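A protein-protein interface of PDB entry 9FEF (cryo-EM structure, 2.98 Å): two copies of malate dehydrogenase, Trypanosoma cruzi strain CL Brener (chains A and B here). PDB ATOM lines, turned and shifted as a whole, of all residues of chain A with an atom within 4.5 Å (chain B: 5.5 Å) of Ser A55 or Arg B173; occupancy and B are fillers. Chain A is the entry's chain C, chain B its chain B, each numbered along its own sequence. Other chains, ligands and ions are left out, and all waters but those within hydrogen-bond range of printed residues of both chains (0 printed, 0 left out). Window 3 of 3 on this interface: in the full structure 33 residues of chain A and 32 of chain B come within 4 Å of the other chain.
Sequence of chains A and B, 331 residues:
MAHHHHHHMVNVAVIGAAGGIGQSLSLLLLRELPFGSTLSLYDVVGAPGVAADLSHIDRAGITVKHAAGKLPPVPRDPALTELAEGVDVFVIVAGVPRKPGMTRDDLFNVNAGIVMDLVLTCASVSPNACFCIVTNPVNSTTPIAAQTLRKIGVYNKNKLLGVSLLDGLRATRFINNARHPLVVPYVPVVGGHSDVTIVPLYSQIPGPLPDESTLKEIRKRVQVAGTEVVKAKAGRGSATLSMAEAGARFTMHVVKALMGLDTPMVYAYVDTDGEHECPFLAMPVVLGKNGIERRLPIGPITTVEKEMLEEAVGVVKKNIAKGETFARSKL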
ATOM      1  N   ALA A  51       6.581 -22.134 -21.763  1.00  0.00           N
ATOM      2  CA  ALA A  51       7.324 -21.331 -20.800  1.00  0.00           C
ATOM      3  C   ALA A  51       8.066 -20.194 -21.487  1.00  0.00           C
ATOM      4  O   ALA A  51       8.016 -19.048 -21.027  1.00  0.00           O
ATOM      5  CB  ALA A  51       8.296 -22.209 -20.020  1.00  0.00           C
ATOM      6  N   ASP A  53       7.350 -18.480 -23.961  1.00  0.00           N
ATOM      7  CA  ASP A  53       6.372 -17.685 -24.691  1.00  0.00           C
ATOM      8  C   ASP A  53       5.782 -16.584 -23.829  1.00  0.00           C
ATOM      9  O   ASP A  53       5.569 -15.471 -24.315  1.00  0.00           O
ATOM     10  CB  ASP A  53       5.254 -18.596 -25.219  1.00  0.00           C
ATOM     11  CG  ASP A  53       4.478 -17.973 -26.355  1.00  0.00           C
ATOM     12  OD1 ASP A  53       4.594 -16.750 -26.565  1.00  0.00           O
ATOM     13  OD2 ASP A  53       3.739 -18.711 -27.040  1.00  0.00           O
ATOM     14  N   LEU A  54       5.525 -16.866 -22.552  1.00  0.00           N
ATOM     15  CA  LEU A  54       5.071 -15.862 -21.602  1.00  0.00           C
ATOM     16  C   LEU A  54       6.223 -15.105 -20.966  1.00  0.00           C
ATOM     17  O   LEU A  54       5.987 -14.089 -20.303  1.00  0.00           O
ATOM     18  CB  LEU A  54       4.226 -16.521 -20.510  1.00  0.00           C
ATOM     19  CG  LEU A  54       3.076 -17.410 -20.976  1.00  0.00           C
ATOM     20  CD1 LEU A  54       2.753 -18.441 -19.914  1.00  0.00           C
ATOM     21  CD2 LEU A  54       1.857 -16.571 -21.298  1.00  0.00           C
ATOM     22  N   SER A  55       7.456 -15.576 -21.147  1.00  0.00           N
ATOM     23  CA  SER A  55       8.615 -14.870 -20.622  1.00  0.00           C
ATOM     24  C   SER A  55       8.957 -13.636 -21.443  1.00  0.00           C
ATOM     25  O   SER A  55       9.738 -12.798 -20.982  1.00  0.00           O
ATOM     26  CB  SER A  55       9.815 -15.812 -20.565  1.00  0.00           C
ATOM     27  OG  SER A  55      10.846 -15.272 -19.761  1.00  0.00           O
ATOM     28  N   HIS A  56       8.401 -13.509 -22.647  1.00  0.00           N
ATOM     29  CA  HIS A  56       8.636 -12.348 -23.492  1.00  0.00           C
ATOM     30  C   HIS A  56       7.611 -11.242 -23.281  1.00  0.00           C
ATOM     31  O   HIS A  56       7.779 -10.152 -23.835  1.00  0.00           O
ATOM     32  CB  HIS A  56       8.648 -12.762 -24.965  1.00  0.00           C
ATOM     33  CG  HIS A  56       9.764 -13.696 -25.319  1.00  0.00           C
ATOM     34  ND1 HIS A  56       9.866 -14.298 -26.554  1.00  0.00           N
ATOM     35  CD2 HIS A  56      10.825 -14.129 -24.600  1.00  0.00           C
ATOM     36  CE1 HIS A  56      10.944 -15.062 -26.580  1.00  0.00           C
ATOM     37  NE2 HIS A  56      11.543 -14.978 -25.406  1.00  0.00           N
ATOM     38  N   ILE A  57       6.560 -11.494 -22.510  1.00  0.00           N
ATOM     39  CA  ILE A  57       5.628 -10.445 -22.113  1.00  0.00           C
ATOM     40  C   ILE A  57       6.243  -9.685 -20.946  1.00  0.00           C
ATOM     41  O   ILE A  57       6.797 -10.295 -20.024  1.00  0.00           O
ATOM     42  CB  ILE A  57       4.263 -11.043 -21.737  1.00  0.00           C
ATOM     43  CG1 ILE A  57       3.719 -11.886 -22.890  1.00  0.00           C
ATOM     44  CG2 ILE A  57       3.282  -9.944 -21.378  1.00  0.00           C
ATOM     45  CD1 ILE A  57       2.337 -12.431 -22.646  1.00  0.00           C
ATOM     46  N   ASP A  58       6.160  -8.353 -20.987  1.00  0.00           N
ATOM     47  CA  ASP A  58       6.918  -7.530 -20.051  1.00  0.00           C
ATOM     48  C   ASP A  58       6.569  -7.839 -18.600  1.00  0.00           C
ATOM     49  O   ASP A  58       7.382  -8.442 -17.895  1.00  0.00           O
ATOM     50  CB  ASP A  58       6.697  -6.046 -20.351  1.00  0.00           C
ATOM     51  CG  ASP A  58       5.281  -5.743 -20.778  1.00  0.00           C
ATOM     52  OD1 ASP A  58       4.397  -6.590 -20.544  1.00  0.00           O
ATOM     53  OD2 ASP A  58       5.051  -4.658 -21.350  1.00  0.00           O
ATOM     54  N   ARG A  59       5.364  -7.466 -18.160  1.00  0.00           N
ATOM     55  CA  ARG A  59       4.835  -7.851 -16.852  1.00  0.00           C
ATOM     56  C   ARG A  59       5.889  -7.790 -15.749  1.00  0.00           C
ATOM     57  O   ARG A  59       6.294  -8.828 -15.217  1.00  0.00           O
ATOM     58  CB  ARG A  59       4.214  -9.248 -16.922  1.00  0.00           C
ATOM     59  CG  ARG A  59       3.417  -9.622 -15.686  1.00  0.00           C
ATOM     60  CD  ARG A  59       2.335  -8.599 -15.415  1.00  0.00           C
ATOM     61  NE  ARG A  59       1.487  -8.983 -14.294  1.00  0.00           N
ATOM     62  CZ  ARG A  59       1.347  -8.268 -13.188  1.00  0.00           C
ATOM     63  NH1 ARG A  59       1.999  -7.131 -13.012  1.00  0.00           N
ATOM     64  NH2 ARG A  59       0.534  -8.703 -12.233  1.00  0.00           N
ATOM     65  N   ILE A  62       7.149 -10.375 -12.100  1.00  0.00           N
ATOM     66  CA  ILE A  62       6.686 -11.757 -12.080  1.00  0.00           C
ATOM     67  C   ILE A  62       7.699 -12.625 -12.811  1.00  0.00           C
ATOM     68  O   ILE A  62       8.074 -12.326 -13.950  1.00  0.00           O
ATOM     69  CB  ILE A  62       5.290 -11.895 -12.714  1.00  0.00           C
ATOM     70  CG1 ILE A  62       4.255 -11.159 -11.869  1.00  0.00           C
ATOM     71  CG2 ILE A  62       4.913 -13.356 -12.868  1.00  0.00           C
ATOM     72  CD1 ILE A  62       2.849 -11.313 -12.373  1.00  0.00           C
ATOM     73  N   GLY B 168       8.265  -4.138 -28.972  1.00  0.00           N
ATOM     74  CA  GLY B 168       8.342  -3.287 -27.797  1.00  0.00           C
ATOM     75  C   GLY B 168       8.179  -4.065 -26.506  1.00  0.00           C
ATOM     76  O   GLY B 168       8.879  -3.807 -25.525  1.00  0.00           O
ATOM     77  N   LEU B 169       7.253  -5.027 -26.491  1.00  0.00           N
ATOM     78  CA  LEU B 169       7.074  -5.871 -25.313  1.00  0.00           C
ATOM     79  C   LEU B 169       8.356  -6.623 -24.980  1.00  0.00           C
ATOM     80  O   LEU B 169       8.798  -6.647 -23.824  1.00  0.00           O
ATOM     81  CB  LEU B 169       5.927  -6.852 -25.550  1.00  0.00           C
ATOM     82  CG  LEU B 169       4.567  -6.555 -24.926  1.00  0.00           C
ATOM     83  CD1 LEU B 169       3.861  -5.455 -25.686  1.00  0.00           C
ATOM     84  CD2 LEU B 169       3.722  -7.811 -24.915  1.00  0.00           C
ATOM     85  N   ARG B 170       8.972  -7.238 -25.991  1.00  0.00           N
ATOM     86  CA  ARG B 170      10.202  -7.990 -25.771  1.00  0.00           C
ATOM     87  C   ARG B 170      11.344  -7.092 -25.318  1.00  0.00           C
ATOM     88  O   ARG B 170      12.097  -7.467 -24.414  1.00  0.00           O
ATOM     89  CB  ARG B 170      10.589  -8.737 -27.044  1.00  0.00           C
ATOM     90  CG  ARG B 170       9.653  -9.872 -27.401  1.00  0.00           C
ATOM     91  CD  ARG B 170      10.334 -10.843 -28.337  1.00  0.00           C
ATOM     92  NE  ARG B 170       9.418 -11.817 -28.916  1.00  0.00           N
ATOM     93  CZ  ARG B 170       9.144 -11.910 -30.209  1.00  0.00           C
ATOM     94  NH1 ARG B 170       9.678 -11.082 -31.090  1.00  0.00           N
ATOM     95  NH2 ARG B 170       8.316 -12.862 -30.629  1.00  0.00           N
ATOM     96  N   ALA B 171      11.491  -5.913 -25.927  1.00  0.00           N
ATOM     97  CA  ALA B 171      12.560  -5.003 -25.527  1.00  0.00           C
ATOM     98  C   ALA B 171      12.368  -4.522 -24.093  1.00  0.00           C
ATOM     99  O   ALA B 171      13.328  -4.459 -23.315  1.00  0.00           O
ATOM    100  CB  ALA B 171      12.629  -3.820 -26.491  1.00  0.00           C
ATOM    101  N   THR B 172      11.131  -4.181 -23.725  1.00  0.00           N
ATOM    102  CA  THR B 172      10.841  -3.759 -22.359  1.00  0.00           C
ATOM    103  C   THR B 172      11.155  -4.871 -21.367  1.00  0.00           C
ATOM    104  O   THR B 172      11.744  -4.629 -20.310  1.00  0.00           O
ATOM    105  CB  THR B 172       9.377  -3.337 -22.241  1.00  0.00           C
ATOM    106  OG1 THR B 172       8.968  -2.679 -23.446  1.00  0.00           O
ATOM    107  CG2 THR B 172       9.188  -2.402 -21.065  1.00  0.00           C
ATOM    108  N   ARG B 173      10.765  -6.102 -21.696  1.00  0.00           N
ATOM    109  CA  ARG B 173      11.047  -7.224 -20.808  1.00  0.00           C
ATOM    110  C   ARG B 173      12.547  -7.451 -20.667  1.00  0.00           C
ATOM    111  O   ARG B 173      13.046  -7.731 -19.571  1.00  0.00           O
ATOM    112  CB  ARG B 173      10.354  -8.484 -21.321  1.00  0.00           C
ATOM    113  CG  ARG B 173      10.637  -9.722 -20.494  1.00  0.00           C
ATOM    114  CD  ARG B 173      10.030  -9.607 -19.111  1.00  0.00           C
ATOM    115  NE  ARG B 173       9.584 -10.896 -18.598  1.00  0.00           N
ATOM    116  CZ  ARG B 173       9.349 -11.152 -17.318  1.00  0.00           C
ATOM    117  NH1 ARG B 173       9.514 -10.228 -16.387  1.00  0.00           N
ATOM    118  NH2 ARG B 173       8.936 -12.366 -16.965  1.00  0.00           N
ATOM    119  N   PHE B 174      13.286  -7.331 -21.772  1.00  0.00           N
ATOM    120  CA  PHE B 174      14.709  -7.654 -21.739  1.00  0.00           C
ATOM    121  C   PHE B 174      15.529  -6.567 -21.057  1.00  0.00           C
ATOM    122  O   PHE B 174      16.576  -6.867 -20.472  1.00  0.00           O
ATOM    123  CB  PHE B 174      15.221  -7.907 -23.157  1.00  0.00           C
ATOM    124  CG  PHE B 174      14.606  -9.109 -23.817  1.00  0.00           C
ATOM    125  CD1 PHE B 174      14.035 -10.117 -23.060  1.00  0.00           C
ATOM    126  CD2 PHE B 174      14.596  -9.231 -25.193  1.00  0.00           C
ATOM    127  CE1 PHE B 174      13.467 -11.218 -23.664  1.00  0.00           C
ATOM    128  CE2 PHE B 174      14.030 -10.331 -25.801  1.00  0.00           C
ATOM    129  CZ  PHE B 174      13.466 -11.325 -25.036  1.00  0.00           C
ATOM    130  N   ILE B 175      15.089  -5.309 -21.117  1.00  0.00           N
ATOM    131  CA  ILE B 175      15.841  -4.268 -20.420  1.00  0.00           C
ATOM    132  C   ILE B 175      15.455  -4.200 -18.946  1.00  0.00           C
ATOM    133  O   ILE B 175      16.277  -3.819 -18.106  1.00  0.00           O
ATOM    134  CB  ILE B 175      15.666  -2.904 -21.109  1.00  0.00           C
ATOM    135  CG1 ILE B 175      16.708  -1.913 -20.587  1.00  0.00           C
ATOM    136  CG2 ILE B 175      14.266  -2.356 -20.891  1.00  0.00           C
ATOM    137  CD1 ILE B 175      18.111  -2.183 -21.074  1.00  0.00           C
ATOM    138  N   ASN B 176      14.220  -4.573 -18.597  1.00  0.00           N
ATOM    139  CA  ASN B 176      13.812  -4.536 -17.197  1.00  0.00           C
ATOM    140  C   ASN B 176      14.513  -5.613 -16.381  1.00  0.00           C
ATOM    141  O   ASN B 176      14.734  -5.430 -15.180  1.00  0.00           O
ATOM    142  CB  ASN B 176      12.297  -4.687 -17.083  1.00  0.00           C
ATOM    143  CG  ASN B 176      11.561  -3.396 -17.357  1.00  0.00           C
ATOM    144  OD1 ASN B 176      12.119  -2.312 -17.225  1.00  0.00           O
ATOM    145  ND2 ASN B 176      10.298  -3.508 -17.737  1.00  0.00           N
ATOM    146  N   ASN B 177      14.864  -6.736 -17.007  1.00  0.00           N
ATOM    147  CA  ASN B 177      15.573  -7.800 -16.310  1.00  0.00           C
ATOM    148  C   ASN B 177      17.026  -7.451 -16.025  1.00  0.00           C
ATOM    149  O   ASN B 177      17.603  -7.989 -15.076  1.00  0.00           O
ATOM    150  CB  ASN B 177      15.515  -9.096 -17.119  1.00  0.00           C
ATOM    151  CG  ASN B 177      14.111  -9.644 -17.242  1.00  0.00           C
ATOM    152  OD1 ASN B 177      13.159  -9.066 -16.722  1.00  0.00           O
ATOM    153  ND2 ASN B 177      13.975 -10.768 -17.933  1.00  0.00           N
ATOM    154  N   ALA B 178      17.628  -6.574 -16.825  1.00  0.00           N
ATOM    155  CA  ALA B 178      19.020  -6.187 -16.652  1.00  0.00           C
ATOM    156  C   ALA B 178      19.189  -4.927 -15.818  1.00  0.00           C
ATOM    157  O   ALA B 178      20.326  -4.518 -15.565  1.00  0.00           O
ATOM    158  CB  ALA B 178      19.685  -5.988 -18.018  1.00  0.00           C
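The backbone carbonyl oxygen (O) of Arg B173 sits close to the side-chain amide oxygen (OD1) of Asn B177 (3.1 Å).
His A56 touches Leu B169.
His A56 touches Arg B173.
His A56 touches Phe B174.
Arg B173 touches Arg A59 (NH1 to O, 3.7 Å).
Hydrophobic or aromatic side chains of chain A within 4 Å of the printed part of chain B: His A56.
Of the 11 printed residues of chain B, 4 touch a printed residue of chain A.
Printed residues of chain B that touch a printed residue of chain A: Leu B169, Arg B170, Arg B173 and Phe B174.
Among the printed residues, no Asp or Glu carboxylate lies within 4 Å of a Lys or Arg side-chain nitrogen of the other chain.
No position is printed for both chains.
Ser A55 touches one residue of chain B.
Of the printed residues of chain B, Ile A62 touches Arg B173.
Of the printed residues of chain A, Arg B170 touches His A56.
Of chain A, only Ser A55 (3.1 Å), His A56 (3.97 Å), Ile A57 (3.2 Å), Asp A58 (3.1 Å), Arg A59 (3.7 Å) and Ile A62 (3.1 Å) come within 4 Å of Arg B173.
The nearest residue of chain B that does not touch Ser A55 is Phe B174 (4.9 Å).
The guanidinium group (NE) of Arg B173 is in hydrogen-bond range of the backbone carbonyl oxygen (O) of Ile A57.
NH2 of Arg B173 sits at hydrogen-bond distance from O of Ile A62.
The guanidinium group (NE) of Arg B170 is in hydrogen-bond range of a ring nitrogen (ND1) of His A56, 3.5 Å away.
The guanidinium group (NE) of Arg B173 lies within hydrogen-bond range of the backbone carbonyl oxygen (O) of Ser A55 (3.1 Å).
NH1 of Arg B173 sits close to O of Asp A58 (3.2 Å).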
